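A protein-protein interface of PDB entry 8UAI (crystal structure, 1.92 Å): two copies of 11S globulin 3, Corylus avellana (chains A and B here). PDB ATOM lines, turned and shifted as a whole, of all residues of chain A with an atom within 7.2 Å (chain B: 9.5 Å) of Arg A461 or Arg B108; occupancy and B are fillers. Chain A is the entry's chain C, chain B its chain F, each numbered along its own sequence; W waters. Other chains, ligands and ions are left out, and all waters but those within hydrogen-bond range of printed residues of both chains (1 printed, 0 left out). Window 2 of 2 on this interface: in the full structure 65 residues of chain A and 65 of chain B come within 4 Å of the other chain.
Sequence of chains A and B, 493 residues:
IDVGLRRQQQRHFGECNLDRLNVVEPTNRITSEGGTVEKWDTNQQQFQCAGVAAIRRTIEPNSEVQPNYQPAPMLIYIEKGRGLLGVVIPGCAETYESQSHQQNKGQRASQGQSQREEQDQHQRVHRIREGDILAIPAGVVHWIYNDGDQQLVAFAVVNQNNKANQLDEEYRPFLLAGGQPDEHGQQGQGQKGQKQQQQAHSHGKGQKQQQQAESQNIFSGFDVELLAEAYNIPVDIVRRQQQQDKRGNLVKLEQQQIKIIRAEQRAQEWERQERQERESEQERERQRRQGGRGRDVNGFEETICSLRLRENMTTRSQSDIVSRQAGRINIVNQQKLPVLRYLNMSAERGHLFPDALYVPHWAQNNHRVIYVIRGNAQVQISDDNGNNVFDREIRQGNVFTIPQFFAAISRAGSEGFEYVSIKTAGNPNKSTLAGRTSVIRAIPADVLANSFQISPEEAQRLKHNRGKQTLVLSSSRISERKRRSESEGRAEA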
ATOM      1  N   SER A 455     -29.670  21.739  29.398  1.00  0.00           N
ATOM      2  CA  SER A 455     -29.318  21.316  30.741  1.00  0.00           C
ATOM      3  C   SER A 455     -27.807  21.326  30.900  1.00  0.00           C
ATOM      4  O   SER A 455     -27.071  21.109  29.930  1.00  0.00           O
ATOM      5  CB  SER A 455     -29.832  19.912  31.038  1.00  0.00           C
ATOM      6  OG  SER A 455     -29.230  18.978  30.159  1.00  0.00           O
ATOM      7  N   PRO A 456     -27.317  21.522  32.123  1.00  0.00           N
ATOM      8  CA  PRO A 456     -25.878  21.347  32.350  1.00  0.00           C
ATOM      9  C   PRO A 456     -25.388  19.981  31.903  1.00  0.00           C
ATOM     10  O   PRO A 456     -24.210  19.845  31.542  1.00  0.00           O
ATOM     11  CB  PRO A 456     -25.714  21.547  33.864  1.00  0.00           C
ATOM     12  CG  PRO A 456     -27.075  21.668  34.435  1.00  0.00           C
ATOM     13  CD  PRO A 456     -28.103  21.564  33.365  1.00  0.00           C
ATOM     14  N   GLU A 457     -26.263  18.965  31.905  1.00  0.00           N
ATOM     15  CA  GLU A 457     -25.897  17.652  31.373  1.00  0.00           C
ATOM     16  C   GLU A 457     -25.644  17.726  29.875  1.00  0.00           C
ATOM     17  O   GLU A 457     -24.671  17.154  29.370  1.00  0.00           O
ATOM     18  CB  GLU A 457     -26.999  16.629  31.653  1.00  0.00           C
ATOM     19  CG  GLU A 457     -26.871  15.894  32.967  1.00  0.00           C
ATOM     20  CD  GLU A 457     -27.277  16.756  34.149  1.00  0.00           C
ATOM     21  OE1 GLU A 457     -27.005  17.974  34.128  1.00  0.00           O
ATOM     22  OE2 GLU A 457     -27.878  16.212  35.101  1.00  0.00           O
ATOM     23  N   GLU A 458     -26.531  18.400  29.142  1.00  0.00           N
ATOM     24  CA  GLU A 458     -26.325  18.592  27.710  1.00  0.00           C
ATOM     25  C   GLU A 458     -25.118  19.462  27.437  1.00  0.00           C
ATOM     26  O   GLU A 458     -24.394  19.233  26.459  1.00  0.00           O
ATOM     27  CB  GLU A 458     -27.572  19.202  27.079  1.00  0.00           C
ATOM     28  CG  GLU A 458     -28.657  18.177  26.775  1.00  0.00           C
ATOM     29  CD  GLU A 458     -29.969  18.819  26.400  1.00  0.00           C
ATOM     30  OE1 GLU A 458     -30.440  19.678  27.186  1.00  0.00           O
ATOM     31  OE2 GLU A 458     -30.515  18.484  25.320  1.00  0.00           O
ATOM     32  N   ALA A 459     -24.861  20.445  28.295  1.00  0.00           N
ATOM     33  CA  ALA A 459     -23.693  21.288  28.083  1.00  0.00           C
ATOM     34  C   ALA A 459     -22.415  20.474  28.214  1.00  0.00           C
ATOM     35  O   ALA A 459     -21.473  20.638  27.425  1.00  0.00           O
ATOM     36  CB  ALA A 459     -23.709  22.462  29.065  1.00  0.00           C
ATOM     37  N   GLN A 460     -22.368  19.583  29.200  1.00  0.00           N
ATOM     38  CA  GLN A 460     -21.206  18.727  29.365  1.00  0.00           C
ATOM     39  C   GLN A 460     -21.004  17.852  28.129  1.00  0.00           C
ATOM     40  O   GLN A 460     -19.891  17.740  27.602  1.00  0.00           O
ATOM     41  CB  GLN A 460     -21.390  17.876  30.619  1.00  0.00           C
ATOM     42  CG  GLN A 460     -21.278  18.655  31.928  1.00  0.00           C
ATOM     43  CD  GLN A 460     -19.857  19.049  32.233  1.00  0.00           C
ATOM     44  OE1 GLN A 460     -18.918  18.519  31.639  1.00  0.00           O
ATOM     45  NE2 GLN A 460     -19.678  19.952  33.190  1.00  0.00           N
ATOM     46  N   ARG A 461     -22.085  17.235  27.642  1.00  0.00           N
ATOM     47  CA  ARG A 461     -21.974  16.391  26.458  1.00  0.00           C
ATOM     48  C   ARG A 461     -21.471  17.182  25.256  1.00  0.00           C
ATOM     49  O   ARG A 461     -20.662  16.673  24.469  1.00  0.00           O
ATOM     50  CB  ARG A 461     -23.316  15.723  26.160  1.00  0.00           C
ATOM     51  CG  ARG A 461     -23.633  14.581  27.119  1.00  0.00           C
ATOM     52  CD  ARG A 461     -25.117  14.246  27.173  1.00  0.00           C
ATOM     53  NE  ARG A 461     -25.744  14.180  25.859  1.00  0.00           N
ATOM     54  CZ  ARG A 461     -25.590  13.183  24.996  1.00  0.00           C
ATOM     55  NH1 ARG A 461     -24.773  12.172  25.247  1.00  0.00           N
ATOM     56  NH2 ARG A 461     -26.295  13.186  23.865  1.00  0.00           N
ATOM     57  N   LEU A 462     -21.934  18.426  25.087  1.00  0.00           N
ATOM     58  CA  LEU A 462     -21.373  19.251  24.013  1.00  0.00           C
ATOM     59  C   LEU A 462     -19.865  19.363  24.134  1.00  0.00           C
ATOM     60  O   LEU A 462     -19.155  19.415  23.121  1.00  0.00           O
ATOM     61  CB  LEU A 462     -21.977  20.651  24.018  1.00  0.00           C
ATOM     62  CG  LEU A 462     -23.390  20.796  23.464  1.00  0.00           C
ATOM     63  CD1 LEU A 462     -23.742  22.279  23.443  1.00  0.00           C
ATOM     64  CD2 LEU A 462     -23.469  20.157  22.076  1.00  0.00           C
ATOM     65  N   LYS A 463     -19.357  19.428  25.367  1.00  0.00           N
ATOM     66  CA  LYS A 463     -17.942  19.704  25.564  1.00  0.00           C
ATOM     67  C   LYS A 463     -17.095  18.448  25.442  1.00  0.00           C
ATOM     68  O   LYS A 463     -15.954  18.530  24.986  1.00  0.00           O
ATOM     69  CB  LYS A 463     -17.708  20.359  26.936  1.00  0.00           C
ATOM     70  CG  LYS A 463     -18.217  21.788  27.034  1.00  0.00           C
ATOM     71  CD  LYS A 463     -18.074  22.389  28.446  1.00  0.00           C
ATOM     72  CE  LYS A 463     -16.620  22.563  28.826  1.00  0.00           C
ATOM     73  NZ  LYS A 463     -16.329  23.781  29.648  1.00  0.00           N
ATOM     74  N   HIS A 464     -17.613  17.276  25.830  1.00  0.00           N
ATOM     75  CA  HIS A 464     -16.761  16.096  25.904  1.00  0.00           C
ATOM     76  C   HIS A 464     -17.185  14.859  25.120  1.00  0.00           C
ATOM     77  O   HIS A 464     -16.426  13.882  25.123  1.00  0.00           O
ATOM     78  CB  HIS A 464     -16.519  15.685  27.370  1.00  0.00           C
ATOM     79  CG  HIS A 464     -16.454  16.838  28.326  1.00  0.00           C
ATOM     80  ND1 HIS A 464     -15.254  17.371  28.748  1.00  0.00           N
ATOM     81  CD2 HIS A 464     -17.420  17.532  28.975  1.00  0.00           C
ATOM     82  CE1 HIS A 464     -15.484  18.362  29.593  1.00  0.00           C
ATOM     83  NE2 HIS A 464     -16.790  18.474  29.753  1.00  0.00           N
ATOM     84  N   ASN A 465     -18.325  14.864  24.425  1.00  0.00           N
ATOM     85  CA  ASN A 465     -18.745  13.625  23.765  1.00  0.00           C
ATOM     86  C   ASN A 465     -17.854  13.271  22.584  1.00  0.00           C
ATOM     87  O   ASN A 465     -17.804  12.103  22.184  1.00  0.00           O
ATOM     88  CB  ASN A 465     -20.207  13.725  23.298  1.00  0.00           C
ATOM     89  CG  ASN A 465     -21.180  13.238  24.341  1.00  0.00           C
ATOM     90  OD1 ASN A 465     -22.346  12.930  24.041  1.00  0.00           O
ATOM     91  ND2 ASN A 465     -20.708  13.140  25.575  1.00  0.00           N
ATOM     92  N   ARG A 466     -17.149  14.248  22.019  1.00  0.00           N
ATOM     93  CA  ARG A 466     -16.287  13.979  20.881  1.00  0.00           C
ATOM     94  C   ARG A 466     -14.909  13.497  21.315  1.00  0.00           C
ATOM     95  O   ARG A 466     -14.136  13.033  20.478  1.00  0.00           O
ATOM     96  CB  ARG A 466     -16.215  15.235  19.998  1.00  0.00           C
ATOM     97  CG  ARG A 466     -15.361  15.108  18.753  1.00  0.00           C
ATOM     98  CD  ARG A 466     -15.704  13.832  17.970  1.00  0.00           C
ATOM     99  NE  ARG A 466     -16.864  13.891  17.079  1.00  0.00           N
ATOM    100  CZ  ARG A 466     -17.099  12.955  16.163  1.00  0.00           C
ATOM    101  NH1 ARG A 466     -16.260  11.945  15.989  1.00  0.00           N
ATOM    102  NH2 ARG A 466     -18.166  13.057  15.372  1.00  0.00           N
ATOM    103  N   GLY A 467     -14.603  13.555  22.609  1.00  0.00           N
ATOM    104  CA  GLY A 467     -13.377  12.934  23.095  1.00  0.00           C
ATOM    105  C   GLY A 467     -12.120  13.597  22.551  1.00  0.00           C
ATOM    106  O   GLY A 467     -12.034  14.822  22.414  1.00  0.00           O
ATOM    107  N   SER A 475     -16.957   9.450  11.847  1.00  0.00           N
ATOM    108  CA  SER A 475     -18.413   9.449  11.932  1.00  0.00           C
ATOM    109  C   SER A 475     -18.850   8.937  13.300  1.00  0.00           C
ATOM    110  O   SER A 475     -18.306   7.961  13.819  1.00  0.00           O
ATOM    111  CB  SER A 475     -19.016   8.573  10.828  1.00  0.00           C
ATOM    112  OG  SER A 475     -20.380   8.298  11.091  1.00  0.00           O
ATOM    113  N   SER A 476     -19.820   9.618  13.905  1.00  0.00           N
ATOM    114  CA  SER A 476     -20.409   9.112  15.139  1.00  0.00           C
ATOM    115  C   SER A 476     -21.544   8.125  14.884  1.00  0.00           C
ATOM    116  O   SER A 476     -22.086   7.566  15.841  1.00  0.00           O
ATOM    117  CB  SER A 476     -20.918  10.275  15.991  1.00  0.00           C
ATOM    118  OG  SER A 476     -22.015  10.873  15.333  1.00  0.00           O
ATOM    119  N   ARG A 477     -21.918   7.893  13.628  1.00  0.00           N
ATOM    120  CA  ARG A 477     -23.086   7.079  13.327  1.00  0.00           C
ATOM    121  C   ARG A 477     -22.828   5.890  12.421  1.00  0.00           C
ATOM    122  O   ARG A 477     -23.693   5.013  12.341  1.00  0.00           O
ATOM    123  CB  ARG A 477     -24.181   7.952  12.702  1.00  0.00           C
ATOM    124  CG  ARG A 477     -24.421   9.223  13.484  1.00  0.00           C
ATOM    125  CD  ARG A 477     -25.696   9.945  13.070  1.00  0.00           C
ATOM    126  NE  ARG A 477     -25.709  10.150  11.631  1.00  0.00           N
ATOM    127  CZ  ARG A 477     -25.938  11.325  11.056  1.00  0.00           C
ATOM    128  NH1 ARG A 477     -26.144  12.423  11.782  1.00  0.00           N
ATOM    129  NH2 ARG A 477     -25.893  11.415   9.725  1.00  0.00           N
ATOM    130  N   GLN B  99      -8.828   7.503  18.888  1.00  0.00           N
ATOM    131  CA  GLN B  99     -10.223   7.388  19.302  1.00  0.00           C
ATOM    132  C   GLN B  99     -11.000   6.526  18.311  1.00  0.00           C
ATOM    133  O   GLN B  99     -10.868   6.680  17.093  1.00  0.00           O
ATOM    134  CB  GLN B  99     -10.854   8.786  19.402  1.00  0.00           C
ATOM    135  CG  GLN B  99     -12.271   8.822  20.023  1.00  0.00           C
ATOM    136  CD  GLN B  99     -12.307   9.071  21.528  1.00  0.00           C
ATOM    137  OE1 GLN B  99     -11.464   9.780  22.087  1.00  0.00           O
ATOM    138  NE2 GLN B  99     -13.310   8.496  22.191  1.00  0.00           N
ATOM    139  N   SER B 100     -11.815   5.617  18.838  1.00  0.00           N
ATOM    140  CA  SER B 100     -12.516   4.631  18.029  1.00  0.00           C
ATOM    141  C   SER B 100     -14.007   4.922  17.994  1.00  0.00           C
ATOM    142  O   SER B 100     -14.535   5.670  18.822  1.00  0.00           O
ATOM    143  CB  SER B 100     -12.287   3.218  18.574  1.00  0.00           C
ATOM    144  OG  SER B 100     -13.052   2.991  19.743  1.00  0.00           O
ATOM    145  N   HIS B 101     -14.683   4.312  17.014  1.00  0.00           N
ATOM    146  CA  HIS B 101     -16.141   4.387  16.961  1.00  0.00           C
ATOM    147  C   HIS B 101     -16.749   3.901  18.268  1.00  0.00           C
ATOM    148  O   HIS B 101     -17.762   4.438  18.734  1.00  0.00           O
ATOM    149  CB  HIS B 101     -16.676   3.574  15.767  1.00  0.00           C
ATOM    150  CG  HIS B 101     -18.177   3.568  15.647  1.00  0.00           C
ATOM    151  ND1 HIS B 101     -18.966   2.541  16.128  1.00  0.00           N
ATOM    152  CD2 HIS B 101     -19.031   4.473  15.103  1.00  0.00           C
ATOM    153  CE1 HIS B 101     -20.239   2.809  15.881  1.00  0.00           C
ATOM    154  NE2 HIS B 101     -20.308   3.979  15.263  1.00  0.00           N
ATOM    155  N   GLN B 102     -16.143   2.882  18.881  1.00  0.00           N
ATOM    156  CA  GLN B 102     -16.753   2.289  20.064  1.00  0.00           C
ATOM    157  C   GLN B 102     -16.642   3.205  21.284  1.00  0.00           C
ATOM    158  O   GLN B 102     -17.558   3.225  22.115  1.00  0.00           O
ATOM    159  CB  GLN B 102     -16.134   0.920  20.338  1.00  0.00           C
ATOM    160  CG  GLN B 102     -16.842   0.110  21.412  1.00  0.00           C
ATOM    161  CD  GLN B 102     -18.355   0.004  21.184  1.00  0.00           C
ATOM    162  OE1 GLN B 102     -19.157   0.275  22.087  1.00  0.00           O
ATOM    163  NE2 GLN B 102     -18.746  -0.399  19.968  1.00  0.00           N
ATOM    164  N   GLN B 103     -15.557   3.985  21.428  1.00  0.00           N
ATOM    165  CA  GLN B 103     -15.580   4.984  22.504  1.00  0.00           C
ATOM    166  C   GLN B 103     -16.520   6.140  22.181  1.00  0.00           C
ATOM    167  O   GLN B 103     -17.187   6.657  23.086  1.00  0.00           O
ATOM    168  CB  GLN B 103     -14.186   5.524  22.876  1.00  0.00           C
ATOM    169  CG  GLN B 103     -13.225   4.485  23.442  1.00  0.00           C
ATOM    170  CD  GLN B 103     -12.166   4.056  22.492  1.00  0.00           C
ATOM    171  OE1 GLN B 103     -11.543   4.888  21.812  1.00  0.00           O
ATOM    172  NE2 GLN B 103     -11.933   2.744  22.428  1.00  0.00           N
ATOM    173  N   ASN B 104     -16.585   6.570  20.914  1.00  0.00           N
ATOM    174  CA  ASN B 104     -17.593   7.552  20.510  1.00  0.00           C
ATOM    175  C   ASN B 104     -18.990   7.095  20.924  1.00  0.00           C
ATOM    176  O   ASN B 104     -19.750   7.843  21.552  1.00  0.00           O
ATOM    177  CB  ASN B 104     -17.561   7.762  18.995  1.00  0.00           C
ATOM    178  CG  ASN B 104     -16.585   8.842  18.550  1.00  0.00           C
ATOM    179  OD1 ASN B 104     -16.134   9.689  19.339  1.00  0.00           O
ATOM    180  ND2 ASN B 104     -16.252   8.815  17.254  1.00  0.00           N
ATOM    181  N   LYS B 105     -19.349   5.871  20.542  1.00  0.00           N
ATOM    182  CA  LYS B 105     -20.684   5.345  20.806  1.00  0.00           C
ATOM    183  C   LYS B 105     -20.901   5.120  22.298  1.00  0.00           C
ATOM    184  O   LYS B 105     -21.969   5.446  22.834  1.00  0.00           O
ATOM    185  CB  LYS B 105     -20.882   4.043  20.023  1.00  0.00           C
ATOM    186  CG  LYS B 105     -22.307   3.773  19.526  1.00  0.00           C
ATOM    187  CD  LYS B 105     -23.008   5.029  19.016  1.00  0.00           C
ATOM    188  CE  LYS B 105     -24.491   4.771  18.745  1.00  0.00           C
ATOM    189  NZ  LYS B 105     -25.338   4.859  19.966  1.00  0.00           N
ATOM    190  N   GLY B 106     -19.897   4.558  22.981  1.00  0.00           N
ATOM    191  CA  GLY B 106     -19.975   4.438  24.425  1.00  0.00           C
ATOM    192  C   GLY B 106     -20.238   5.769  25.098  1.00  0.00           C
ATOM    193  O   GLY B 106     -21.080   5.868  25.990  1.00  0.00           O
ATOM    194  N   GLN B 107     -19.529   6.817  24.664  1.00  0.00           N
ATOM    195  CA  GLN B 107     -19.707   8.143  25.251  1.00  0.00           C
ATOM    196  C   GLN B 107     -21.135   8.646  25.061  1.00  0.00           C
ATOM    197  O   GLN B 107     -21.816   8.999  26.033  1.00  0.00           O
ATOM    198  CB  GLN B 107     -18.700   9.132  24.642  1.00  0.00           C
ATOM    199  CG  GLN B 107     -17.615   9.598  25.604  1.00  0.00           C
ATOM    200  CD  GLN B 107     -16.325  10.077  24.923  1.00  0.00           C
ATOM    201  OE1 GLN B 107     -16.127   9.936  23.703  1.00  0.00           O
ATOM    202  NE2 GLN B 107     -15.429  10.631  25.725  1.00  0.00           N
ATOM    203  N   ARG B 108     -21.609   8.699  23.810  1.00  0.00           N
ATOM    204  CA  ARG B 108     -22.931   9.270  23.553  1.00  0.00           C
ATOM    205  C   ARG B 108     -24.043   8.453  24.203  1.00  0.00           C
ATOM    206  O   ARG B 108     -25.032   9.028  24.680  1.00  0.00           O
ATOM    207  CB  ARG B 108     -23.181   9.392  22.051  1.00  0.00           C
ATOM    208  CG  ARG B 108     -24.473  10.108  21.697  1.00  0.00           C
ATOM    209  CD  ARG B 108     -25.117   9.476  20.480  1.00  0.00           C
ATOM    210  NE  ARG B 108     -24.787  10.217  19.270  1.00  0.00           N
ATOM    211  CZ  ARG B 108     -24.881   9.723  18.041  1.00  0.00           C
ATOM    212  NH1 ARG B 108     -25.316   8.490  17.823  1.00  0.00           N
ATOM    213  NH2 ARG B 108     -24.499  10.478  17.008  1.00  0.00           N
ATOM    214  N   ALA B 109     -23.906   7.118  24.237  1.00  0.00           N
ATOM    215  CA  ALA B 109     -24.892   6.292  24.939  1.00  0.00           C
ATOM    216  C   ALA B 109     -24.935   6.570  26.461  1.00  0.00           C
ATOM    217  O   ALA B 109     -25.658   5.860  27.171  1.00  0.00           O
ATOM    218  CB  ALA B 109     -24.605   4.812  24.693  1.00  0.00           C
ATOM    219  N   SER B 110     -24.190   7.568  26.945  1.00  0.00           N
ATOM    220  CA  SER B 110     -24.148   7.935  28.366  1.00  0.00           C
ATOM    221  C   SER B 110     -23.462   6.853  29.191  1.00  0.00           C
ATOM    222  O   SER B 110     -23.314   5.719  28.735  1.00  0.00           O
ATOM    223  CB  SER B 110     -25.556   8.199  28.903  1.00  0.00           C
ATOM    224  OG  SER B 110     -25.905   9.565  28.756  1.00  0.00           O
ATOM    225  N   GLN B 113     -21.286  11.384  30.163  1.00  0.00           N
ATOM    226  CA  GLN B 113     -20.233  11.840  29.257  1.00  0.00           C
ATOM    227  C   GLN B 113     -19.943  13.327  29.476  1.00  0.00           C
ATOM    228  O   GLN B 113     -20.716  14.188  29.057  1.00  0.00           O
ATOM    229  N   SER B 114     -18.824  13.632  30.131  1.00  0.00           N
ATOM    230  CA  SER B 114     -18.531  15.011  30.500  1.00  0.00           C
ATOM    231  C   SER B 114     -17.098  15.157  31.002  1.00  0.00           C
ATOM    232  O   SER B 114     -16.154  14.716  30.335  1.00  0.00           O
ATOM    233  CB  SER B 114     -19.529  15.497  31.555  1.00  0.00           C
ATOM    234  OG  SER B 114     -19.726  14.536  32.582  1.00  0.00           O
ATOM    235  N   GLN B 115     -16.921  15.801  32.158  1.00  0.00           N
ATOM    236  CA  GLN B 115     -15.596  15.893  32.762  1.00  0.00           C
ATOM    237  C   GLN B 115     -15.319  14.770  33.756  1.00  0.00           C
ATOM    238  O   GLN B 115     -14.311  14.071  33.627  1.00  0.00           O
ATOM    239  CB  GLN B 115     -15.397  17.246  33.437  1.00  0.00           C
ATOM    240  CG  GLN B 115     -14.094  17.302  34.205  1.00  0.00           C
ATOM    241  CD  GLN B 115     -13.559  18.687  34.310  1.00  0.00           C
ATOM    242  OE1 GLN B 115     -13.861  19.540  33.478  1.00  0.00           O
ATOM    243  NE2 GLN B 115     -12.798  18.951  35.366  1.00  0.00           N
HETATM  244  O   HOH W   1     -22.070   7.777  18.700  1.00  0.00           O
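The backbone carbonyl oxygen of Asn A465 sits close to the side-chain amide oxygen of Gln B107. NH1 of Arg A466 sits close to ND2 of Asn B104 (3.4 Å). O of Ser B114 sits close to ND1 of His A464. O of His A464 sits at hydrogen-bond distance from NE2 of Gln B107, 3.5 Å away. OG of Ser A476 sits at hydrogen-bond distance from NH2 of Arg B108. The guanidinium group (NH1) of Arg A461 sits at hydrogen-bond distance from the backbone carbonyl oxygen (O) of Arg B108 (3.2 Å). The side-chain amide oxygen (OE1) of Gln A460 lies within hydrogen-bond range of the backbone NH (N) of Gln B115, 3.4 Å away.
Of the 16 printed residues of chain A, 9 touch a printed residue of chain B. Of the 15 printed residues of chain B, 8 touch a printed residue of chain A. Among the printed residues, 16 pairs touch across the chains. Among the printed residues, no Asp or Glu carboxylate lies within 4 Å of a Lys or Arg side-chain nitrogen of the other chain.
The side-chain hydroxyl (OG) of Ser A475 is in hydrogen-bond range of the backbone NH (N) of Arg A477 (3.0 Å). OE1 of Gln A460 is in hydrogen-bond range of NE2 of His A464. NH1 of Arg A461 is in hydrogen-bond range of OD1 of Asn A465 (2.8 Å).
Water W1 bridges O of Ser A476 (2.9 Å) and NH1 of Arg B108 (3.4 Å).
O of Gln B113 touches C of Gln A460, 3.8 Å away. Ser B114 touches Gln A460 (CB to OE1, 3.1 Å). CG of Arg A461 touches O of Gln B113, at 3.5 Å. N of Gln B115 touches NE2 of His A464 (3.6 Å). Arg B108 touches Asn A465. Asn A465 touches Gln B113 (ND2 to O, 3.6 Å). Gly A467 touches Gln B99 (CA to OE1, 3.8 Å). O of Ser A475 touches CD2 of His B101 (3.8 Å). Arg B108 touches Arg A477 (NH2 to CG, 3.7 Å).
No position is printed for both chains. Of the 16 pairs that touch across the chains among the printed residues, none has its exchanged pair printed and touching as well.
Printed residues of chain B within 4 Å of Arg A461: Arg B108 and Gln B113. Leu A462 touches none of the printed residues of chain B. Of chain B, only Gln B107, Arg B108 and Gln B113 come within 4 Å of Asn A465. Of the printed residues of chain B, Arg A466 touches Asn B104 (3.4 Å). Printed residues of chain A within 4 Å of Gln B99: Gly A467 (3.8 Å). Printed residues of chain A within 4 Å of His B101: Ser A475. Of the printed residues of chain A, Asn B104 touches Arg A466 (3.4 Å). Of the printed residues of chain A, Arg B108 touches Arg A461, Asn A465, Ser A476 and Arg A477. Of the printed residues of chain A, Gln B115 touches Gln A460 (3.4 Å) and His A464 (3.6 Å). The nearest printed residue of chain B that does not touch His A464 is Gln B113 (4.7 Å).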
